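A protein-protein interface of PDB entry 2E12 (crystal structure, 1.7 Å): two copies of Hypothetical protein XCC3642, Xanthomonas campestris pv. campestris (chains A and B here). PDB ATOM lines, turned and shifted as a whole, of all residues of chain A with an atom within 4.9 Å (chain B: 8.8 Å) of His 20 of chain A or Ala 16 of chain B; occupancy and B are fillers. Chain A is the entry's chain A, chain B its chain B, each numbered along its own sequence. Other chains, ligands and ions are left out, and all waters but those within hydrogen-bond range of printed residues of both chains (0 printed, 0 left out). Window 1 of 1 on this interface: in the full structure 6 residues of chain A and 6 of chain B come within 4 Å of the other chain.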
ATOM      1  N   ALA A  16      19.250  -8.107 -18.128  1.00  0.00           N
ATOM      2  CA  ALA A  16      18.651  -7.061 -18.962  1.00  0.00           C
ATOM      3  C   ALA A  16      19.335  -7.042 -20.330  1.00  0.00           C
ATOM      4  O   ALA A  16      18.679  -6.887 -21.362  1.00  0.00           O
ATOM      5  CB  ALA A  16      18.790  -5.694 -18.285  1.00  0.00           C
ATOM      6  N   THR A  17      20.654  -7.203 -20.332  1.00  0.00           N
ATOM      7  CA  THR A  17      21.417  -7.230 -21.574  1.00  0.00           C
ATOM      8  C   THR A  17      21.016  -8.472 -22.378  1.00  0.00           C
ATOM      9  O   THR A  17      20.663  -8.367 -23.551  1.00  0.00           O
ATOM     10  CB  THR A  17      22.945  -7.266 -21.302  1.00  0.00           C
ATOM     11  OG1 THR A  17      23.268  -8.419 -20.521  1.00  0.00           O
ATOM     12  CG2 THR A  17      23.374  -6.033 -20.530  1.00  0.00           C
ATOM     13  N   LEU A  18      21.049  -9.638 -21.733  1.00  0.00           N
ATOM     14  CA  LEU A  18      20.684 -10.886 -22.394  1.00  0.00           C
ATOM     15  C   LEU A  18      19.307 -10.840 -23.049  1.00  0.00           C
ATOM     16  O   LEU A  18      19.115 -11.395 -24.132  1.00  0.00           O
ATOM     17  CB  LEU A  18      20.737 -12.050 -21.395  1.00  0.00           C
ATOM     18  CG  LEU A  18      22.127 -12.488 -20.921  1.00  0.00           C
ATOM     19  CD1 LEU A  18      22.003 -13.475 -19.770  1.00  0.00           C
ATOM     20  CD2 LEU A  18      22.881 -13.118 -22.084  1.00  0.00           C
ATOM     21  N   GLU A  19      18.351 -10.180 -22.400  1.00  0.00           N
ATOM     22  CA  GLU A  19      16.994 -10.096 -22.938  1.00  0.00           C
ATOM     23  C   GLU A  19      16.861  -9.147 -24.122  1.00  0.00           C
ATOM     24  O   GLU A  19      16.091  -9.410 -25.046  1.00  0.00           O
ATOM     25  CB  GLU A  19      16.008  -9.708 -21.821  1.00  0.00           C
ATOM     26  CG  GLU A  19      15.787 -10.831 -20.810  1.00  0.00           C
ATOM     27  CD  GLU A  19      14.925 -10.417 -19.629  1.00  0.00           C
ATOM     28  OE1 GLU A  19      15.289  -9.447 -18.932  1.00  0.00           O
ATOM     29  OE2 GLU A  19      13.888 -11.071 -19.388  1.00  0.00           O
ATOM     30  N   HIS A  20      17.612  -8.046 -24.102  1.00  0.00           N
ATOM     31  CA  HIS A  20      17.560  -7.085 -25.203  1.00  0.00           C
ATOM     32  C   HIS A  20      18.090  -7.719 -26.498  1.00  0.00           C
ATOM     33  O   HIS A  20      17.593  -7.427 -27.575  1.00  0.00           O
ATOM     34  CB  HIS A  20      18.382  -5.835 -24.866  1.00  0.00           C
ATOM     35  CG  HIS A  20      18.362  -4.790 -25.939  1.00  0.00           C
ATOM     36  ND1 HIS A  20      17.205  -4.157 -26.339  1.00  0.00           N
ATOM     37  CD2 HIS A  20      19.356  -4.274 -26.699  1.00  0.00           C
ATOM     38  CE1 HIS A  20      17.488  -3.296 -27.302  1.00  0.00           C
ATOM     39  NE2 HIS A  20      18.786  -3.349 -27.539  1.00  0.00           N
ATOM     40  N   TRP A  21      19.089  -8.594 -26.377  1.00  0.00           N
ATOM     41  CA  TRP A  21      19.679  -9.265 -27.538  1.00  0.00           C
ATOM     42  C   TRP A  21      18.660 -10.130 -28.264  1.00  0.00           C
ATOM     43  O   TRP A  21      18.663 -10.209 -29.495  1.00  0.00           O
ATOM     44  CB  TRP A  21      20.864 -10.145 -27.115  1.00  0.00           C
ATOM     45  CG  TRP A  21      22.103  -9.391 -26.688  1.00  0.00           C
ATOM     46  CD1 TRP A  21      23.102  -9.856 -25.881  1.00  0.00           C
ATOM     47  CD2 TRP A  21      22.481  -8.058 -27.064  1.00  0.00           C
ATOM     48  NE1 TRP A  21      24.074  -8.900 -25.728  1.00  0.00           N
ATOM     49  CE2 TRP A  21      23.720  -7.787 -26.443  1.00  0.00           C
ATOM     50  CE3 TRP A  21      21.894  -7.067 -27.864  1.00  0.00           C
ATOM     51  CZ2 TRP A  21      24.384  -6.565 -26.596  1.00  0.00           C
ATOM     52  CZ3 TRP A  21      22.554  -5.852 -28.015  1.00  0.00           C
ATOM     53  CH2 TRP A  21      23.787  -5.614 -27.383  1.00  0.00           C
ATOM     54  N   VAL A  22      17.800 -10.795 -27.499  1.00  0.00           N
ATOM     55  CA  VAL A  22      16.771 -11.642 -28.090  1.00  0.00           C
ATOM     56  C   VAL A  22      15.853 -10.779 -28.959  1.00  0.00           C
ATOM     57  O   VAL A  22      15.522 -11.143 -30.076  1.00  0.00           O
ATOM     58  CB  VAL A  22      15.946 -12.360 -26.988  1.00  0.00           C
ATOM     59  CG1 VAL A  22      14.854 -13.227 -27.610  1.00  0.00           C
ATOM     60  CG2 VAL A  22      16.878 -13.218 -26.131  1.00  0.00           C
ATOM     61  N   LYS A  23      15.470  -9.623 -28.427  1.00  0.00           N
ATOM     62  CA  LYS A  23      14.614  -8.674 -29.128  1.00  0.00           C
ATOM     63  C   LYS A  23      15.217  -8.260 -30.469  1.00  0.00           C
ATOM     64  O   LYS A  23      14.497  -7.931 -31.412  1.00  0.00           O
ATOM     65  CB  LYS A  23      14.406  -7.427 -28.260  1.00  0.00           C
ATOM     66  CG  LYS A  23      13.477  -7.622 -27.072  1.00  0.00           C
ATOM     67  CD  LYS A  23      12.023  -7.632 -27.508  1.00  0.00           C
ATOM     68  CE  LYS A  23      11.725  -6.414 -28.372  1.00  0.00           C
ATOM     69  NZ  LYS A  23      12.307  -5.176 -27.778  1.00  0.00           N
ATOM     70  N   LEU A  24      16.542  -8.268 -30.546  1.00  0.00           N
ATOM     71  CA  LEU A  24      17.234  -7.890 -31.767  1.00  0.00           C
ATOM     72  C   LEU A  24      17.649  -9.101 -32.608  1.00  0.00           C
ATOM     73  O   LEU A  24      18.218  -8.946 -33.683  1.00  0.00           O
ATOM     74  CB  LEU A  24      18.463  -7.054 -31.422  1.00  0.00           C
ATOM     75  CG  LEU A  24      18.187  -5.802 -30.582  1.00  0.00           C
ATOM     76  CD1 LEU A  24      19.508  -5.106 -30.274  1.00  0.00           C
ATOM     77  CD2 LEU A  24      17.243  -4.865 -31.323  1.00  0.00           C
ATOM     78  N   TYR B   9      17.785   9.199 -24.638  1.00  0.00           N
ATOM     79  CA  TYR B   9      18.850   8.209 -24.863  1.00  0.00           C
ATOM     80  C   TYR B   9      18.657   7.321 -26.099  1.00  0.00           C
ATOM     81  O   TYR B   9      17.534   6.945 -26.430  1.00  0.00           O
ATOM     82  CB  TYR B   9      18.968   7.300 -23.636  1.00  0.00           C
ATOM     83  CG  TYR B   9      19.174   8.044 -22.339  1.00  0.00           C
ATOM     84  CD1 TYR B   9      20.445   8.456 -21.939  1.00  0.00           C
ATOM     85  CD2 TYR B   9      18.090   8.361 -21.522  1.00  0.00           C
ATOM     86  CE1 TYR B   9      20.630   9.164 -20.753  1.00  0.00           C
ATOM     87  CE2 TYR B   9      18.264   9.068 -20.342  1.00  0.00           C
ATOM     88  CZ  TYR B   9      19.531   9.466 -19.960  1.00  0.00           C
ATOM     89  OH  TYR B   9      19.694  10.157 -18.781  1.00  0.00           O
ATOM     90  N   THR B  10      19.758   6.969 -26.771  1.00  0.00           N
ATOM     91  CA  THR B  10      19.682   6.107 -27.959  1.00  0.00           C
ATOM     92  C   THR B  10      20.669   4.933 -27.992  1.00  0.00           C
ATOM     93  O   THR B  10      20.671   4.173 -28.948  1.00  0.00           O
ATOM     94  CB  THR B  10      19.884   6.909 -29.273  1.00  0.00           C
ATOM     95  OG1 THR B  10      21.185   7.501 -29.274  1.00  0.00           O
ATOM     96  CG2 THR B  10      18.830   8.004 -29.404  1.00  0.00           C
ATOM     97  N   GLU B  11      21.496   4.761 -26.966  1.00  0.00           N
ATOM     98  CA  GLU B  11      22.455   3.649 -26.981  1.00  0.00           C
ATOM     99  C   GLU B  11      21.790   2.322 -26.618  1.00  0.00           C
ATOM    100  O   GLU B  11      21.021   2.267 -25.678  1.00  0.00           O
ATOM    101  CB  GLU B  11      23.616   3.928 -26.021  1.00  0.00           C
ATOM    102  CG  GLU B  11      24.692   4.842 -26.591  1.00  0.00           C
ATOM    103  CD  GLU B  11      25.926   4.897 -25.714  1.00  0.00           C
ATOM    104  OE1 GLU B  11      25.865   5.513 -24.629  1.00  0.00           O
ATOM    105  OE2 GLU B  11      26.959   4.313 -26.109  1.00  0.00           O
ATOM    106  N   GLN B  12      22.091   1.256 -27.362  1.00  0.00           N
ATOM    107  CA  GLN B  12      21.495  -0.062 -27.102  1.00  0.00           C
ATOM    108  C   GLN B  12      21.518  -0.509 -25.636  1.00  0.00           C
ATOM    109  O   GLN B  12      20.522  -1.042 -25.135  1.00  0.00           O
ATOM    110  CB  GLN B  12      22.178  -1.132 -27.965  1.00  0.00           C
ATOM    111  CG  GLN B  12      21.995  -0.926 -29.459  1.00  0.00           C
ATOM    112  CD  GLN B  12      20.532  -0.876 -29.850  1.00  0.00           C
ATOM    113  OE1 GLN B  12      19.778  -1.811 -29.585  1.00  0.00           O
ATOM    114  NE2 GLN B  12      20.123   0.217 -30.482  1.00  0.00           N
ATOM    115  N   ALA B  13      22.650  -0.324 -24.957  1.00  0.00           N
ATOM    116  CA  ALA B  13      22.757  -0.705 -23.548  1.00  0.00           C
ATOM    117  C   ALA B  13      21.747   0.110 -22.756  1.00  0.00           C
ATOM    118  O   ALA B  13      21.042  -0.422 -21.902  1.00  0.00           O
ATOM    119  CB  ALA B  13      24.161  -0.437 -23.028  1.00  0.00           C
ATOM    120  N   GLN B  14      21.678   1.406 -23.051  1.00  0.00           N
ATOM    121  CA  GLN B  14      20.730   2.280 -22.371  1.00  0.00           C
ATOM    122  C   GLN B  14      19.311   1.781 -22.598  1.00  0.00           C
ATOM    123  O   GLN B  14      18.523   1.703 -21.664  1.00  0.00           O
ATOM    124  CB  GLN B  14      20.852   3.710 -22.884  1.00  0.00           C
ATOM    125  CG  GLN B  14      22.250   4.290 -22.757  1.00  0.00           C
ATOM    126  CD  GLN B  14      22.325   5.722 -23.238  1.00  0.00           C
ATOM    127  OE1 GLN B  14      21.874   6.046 -24.340  1.00  0.00           O
ATOM    128  NE2 GLN B  14      22.902   6.592 -22.416  1.00  0.00           N
ATOM    129  N   ILE B  15      18.997   1.462 -23.848  1.00  0.00           N
ATOM    130  CA  ILE B  15      17.683   0.951 -24.207  1.00  0.00           C
ATOM    131  C   ILE B  15      17.419  -0.331 -23.409  1.00  0.00           C
ATOM    132  O   ILE B  15      16.335  -0.516 -22.862  1.00  0.00           O
ATOM    133  CB  ILE B  15      17.601   0.643 -25.732  1.00  0.00           C
ATOM    134  CG1 ILE B  15      17.775   1.930 -26.540  1.00  0.00           C
ATOM    135  CG2 ILE B  15      16.268  -0.015 -26.066  1.00  0.00           C
ATOM    136  CD1 ILE B  15      17.721   1.728 -28.054  1.00  0.00           C
ATOM    137  N   ALA B  16      18.429  -1.199 -23.344  1.00  0.00           N
ATOM    138  CA  ALA B  16      18.346  -2.469 -22.622  1.00  0.00           C
ATOM    139  C   ALA B  16      17.875  -2.254 -21.190  1.00  0.00           C
ATOM    140  O   ALA B  16      17.030  -2.989 -20.689  1.00  0.00           O
ATOM    141  CB  ALA B  16      19.719  -3.163 -22.624  1.00  0.00           C
ATOM    142  N   THR B  17      18.440  -1.237 -20.548  1.00  0.00           N
ATOM    143  CA  THR B  17      18.114  -0.872 -19.172  1.00  0.00           C
ATOM    144  C   THR B  17      16.658  -0.420 -19.031  1.00  0.00           C
ATOM    145  O   THR B  17      15.937  -0.869 -18.132  1.00  0.00           O
ATOM    146  CB  THR B  17      19.025   0.289 -18.678  1.00  0.00           C
ATOM    147  OG1 THR B  17      20.393  -0.141 -18.651  1.00  0.00           O
ATOM    148  CG2 THR B  17      18.607   0.752 -17.279  1.00  0.00           C
ATOM    149  N   LEU B  18      16.230   0.468 -19.923  1.00  0.00           N
ATOM    150  CA  LEU B  18      14.867   0.995 -19.881  1.00  0.00           C
ATOM    151  C   LEU B  18      13.821  -0.088 -20.095  1.00  0.00           C
ATOM    152  O   LEU B  18      12.778  -0.095 -19.449  1.00  0.00           O
ATOM    153  CB  LEU B  18      14.691   2.113 -20.921  1.00  0.00           C
ATOM    154  CG  LEU B  18      15.497   3.394 -20.685  1.00  0.00           C
ATOM    155  CD1 LEU B  18      15.136   4.416 -21.749  1.00  0.00           C
ATOM    156  CD2 LEU B  18      15.207   3.955 -19.305  1.00  0.00           C
ATOM    157  N   GLU B  19      14.108  -1.009 -21.006  1.00  0.00           N
ATOM    158  CA  GLU B  19      13.196  -2.096 -21.305  1.00  0.00           C
ATOM    159  C   GLU B  19      13.137  -3.083 -20.143  1.00  0.00           C
ATOM    160  O   GLU B  19      12.132  -3.760 -19.957  1.00  0.00           O
ATOM    161  CB  GLU B  19      13.649  -2.836 -22.566  1.00  0.00           C
ATOM    162  CG  GLU B  19      13.711  -1.989 -23.833  1.00  0.00           C
ATOM    163  CD  GLU B  19      14.298  -2.754 -25.015  1.00  0.00           C
ATOM    164  OE1 GLU B  19      14.296  -2.210 -26.140  1.00  0.00           O
ATOM    165  OE2 GLU B  19      14.769  -3.895 -24.818  1.00  0.00           O
ATOM    166  N   HIS B  20      14.219  -3.189 -19.378  1.00  0.00           N
ATOM    167  CA  HIS B  20      14.220  -4.123 -18.262  1.00  0.00           C
ATOM    168  C   HIS B  20      13.414  -3.530 -17.119  1.00  0.00           C
ATOM    169  O   HIS B  20      12.785  -4.256 -16.345  1.00  0.00           O
ATOM    170  CB  HIS B  20      15.647  -4.434 -17.811  1.00  0.00           C
ATOM    171  CG  HIS B  20      15.726  -5.492 -16.755  1.00  0.00           C
ATOM    172  ND1 HIS B  20      15.214  -6.759 -16.933  1.00  0.00           N
ATOM    173  CD2 HIS B  20      16.249  -5.470 -15.506  1.00  0.00           C
ATOM    174  CE1 HIS B  20      15.418  -7.472 -15.839  1.00  0.00           C
ATOM    175  NE2 HIS B  20      16.046  -6.713 -14.958  1.00  0.00           N
ATOM    176  N   TRP B  21      13.417  -2.203 -17.039  1.00  0.00           N
ATOM    177  CA  TRP B  21      12.677  -1.494 -16.007  1.00  0.00           C
ATOM    178  C   TRP B  21      11.184  -1.658 -16.251  1.00  0.00           C
ATOM    179  O   TRP B  21      10.424  -1.897 -15.321  1.00  0.00           O
ATOM    180  CB  TRP B  21      13.047  -0.008 -16.005  1.00  0.00           C
ATOM    181  CG  TRP B  21      14.325   0.308 -15.302  1.00  0.00           C
ATOM    182  CD1 TRP B  21      15.120   1.398 -15.503  1.00  0.00           C
ATOM    183  CD2 TRP B  21      14.937  -0.449 -14.250  1.00  0.00           C
ATOM    184  NE1 TRP B  21      16.191   1.368 -14.642  1.00  0.00           N
ATOM    185  CE2 TRP B  21      16.103   0.244 -13.862  1.00  0.00           C
ATOM    186  CE3 TRP B  21      14.615  -1.648 -13.595  1.00  0.00           C
ATOM    187  CZ2 TRP B  21      16.949  -0.219 -12.849  1.00  0.00           C
ATOM    188  CZ3 TRP B  21      15.454  -2.109 -12.588  1.00  0.00           C
ATOM    189  CH2 TRP B  21      16.608  -1.395 -12.225  1.00  0.00           C
ATOM    190  N   VAL B  22      10.780  -1.539 -17.510  1.00  0.00           N
ATOM    191  CA  VAL B  22       9.381  -1.689 -17.885  1.00  0.00           C
ATOM    192  C   VAL B  22       8.895  -3.101 -17.573  1.00  0.00           C
ATOM    193  O   VAL B  22       7.701  -3.324 -17.363  1.00  0.00           O
ATOM    194  CB  VAL B  22       9.166  -1.423 -19.394  1.00  0.00           C
ATOM    195  CG1 VAL B  22       7.708  -1.678 -19.768  1.00  0.00           C
ATOM    196  CG2 VAL B  22       9.555   0.014 -19.733  1.00  0.00           C
ATOM    197  N   LYS B  23       9.819  -4.055 -17.547  1.00  0.00           N
ATOM    198  CA  LYS B  23       9.456  -5.436 -17.263  1.00  0.00           C
ATOM    199  C   LYS B  23       9.223  -5.657 -15.768  1.00  0.00           C
ATOM    200  O   LYS B  23       8.226  -6.272 -15.382  1.00  0.00           O
ATOM    201  CB  LYS B  23      10.547  -6.381 -17.774  1.00  0.00           C
ATOM    202  CG  LYS B  23      10.179  -7.863 -17.700  1.00  0.00           C
ATOM    203  CD  LYS B  23      11.196  -8.729 -18.435  1.00  0.00           C
ATOM    204  CE  LYS B  23      11.256  -8.368 -19.912  1.00  0.00           C
ATOM    205  NZ  LYS B  23      12.159  -9.266 -20.681  1.00  0.00           N
ATOM    206  N   ILE B  51       7.994   3.197 -22.815  1.00  0.00           N
ATOM    207  CA  ILE B  51       9.044   3.962 -23.470  1.00  0.00           C
ATOM    208  C   ILE B  51       8.446   4.736 -24.641  1.00  0.00           C
ATOM    209  O   ILE B  51       7.605   4.214 -25.368  1.00  0.00           O
ATOM    210  CB  ILE B  51      10.171   3.044 -23.979  1.00  0.00           C
ATOM    211  CG1 ILE B  51      10.693   2.173 -22.829  1.00  0.00           C
ATOM    212  CG2 ILE B  51      11.315   3.892 -24.534  1.00  0.00           C
ATOM    213  CD1 ILE B  51      11.767   1.183 -23.234  1.00  0.00           C
ATOM    214  N   SER B  63      14.957   8.140 -26.570  1.00  0.00           N
ATOM    215  CA  SER B  63      13.983   7.396 -25.769  1.00  0.00           C
ATOM    216  C   SER B  63      14.051   7.725 -24.272  1.00  0.00           C
ATOM    217  O   SER B  63      15.105   8.088 -23.739  1.00  0.00           O
ATOM    218  CB  SER B  63      14.206   5.889 -25.935  1.00  0.00           C
ATOM    219  OG  SER B  63      14.154   5.473 -27.290  1.00  0.00           O
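His 20 of chain B touches Ala 16 of chain A.
Ile 15 of chain B touches His 20 of chain A (CG2 to CE1, 3.7 Å).
Ala 16 of chain B touches His 20 of chain A.
Gln 12 of chain B touches Leu 24 of chain A.
His 20 of chain A touches just these residues of chain B: Gln 12 (2.7 Å), Ile 15 (3.7 Å), Ala 16 (3.7 Å) and Glu 19 (2.9 Å).
Printed residues of chain B within 4 Å of Lys 23 of chain A: Glu 19 (3.9 Å).
Ala 13 of chain B touches none of the printed residues of chain A.
Ala 16 of chain B touches just one residue of chain A: His 20 (3.7 Å).
Printed residues of chain A within 4 Å of Glu 19 of chain B: His 20 (2.9 Å) and Lys 23 (3.9 Å).
Of the printed residues of chain A, His 20 of chain B touches Ala 16 and Glu 19.
Printed residues of chain A within 4 Å of Lys 23 of chain B: Glu 19.
The nearest residue of chain B that does not touch His 20 of chain A is Ala 13 of chain B (5.4 Å).
ND1 of His 20 of chain B is in hydrogen-bond range of OE1 of Glu 19 of chain A, at 3.4 Å.
The side-chain carboxylate (OE2) of Glu 19 of chain A lies within salt-bridge range of the side-chain amino group (NZ) of Lys 23 of chain B, at 2.8 Å.
OE1 of Gln 12 of chain B is in hydrogen-bond range of NE2 of His 20 of chain A.
OE2 of Glu 19 of chain B lies within hydrogen-bond range of ND1 of His 20 of chain A, 2.9 Å away.
The side-chain amino group of Lys 23 of chain A is in salt-bridge range of the side-chain carboxylate of Glu 19 of chain B, at 3.9 Å.
Ala 16 of chain A touches His 20 of chain B, and with the chains exchanged His 20 of chain A touches Ala 16 of chain B.
Glu 19 of chain A touches His 20 of chain B, and with the chains exchanged His 20 of chain A touches Glu 19 of chain B.
Glu 19 of chain A touches Lys 23 of chain B, and with the chains exchanged Lys 23 of chain A touches Glu 19 of chain B.
8 positions are printed for both chains.
Printed residues of chain A that touch a printed residue of chain B: Ala 16, Glu 19, His 20, Lys 23 and Leu 24.
Along chain A the printed residues that touch a printed residue of chain B span positions 16 to 24.
Hydrophobic or aromatic side chains of chain B that line the printed part of chain A: Ile 15, Ala 16 and His 20.
Among the printed residues, 9 pairs touch across the chains.
Among the printed residues, Asp or Glu carboxylates within 4 Å of a Lys or Arg side-chain nitrogen of the other chain: Glu 19 of chain A with Lys 23 of chain B and Lys 23 of chain A with Glu 19 of chain B.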
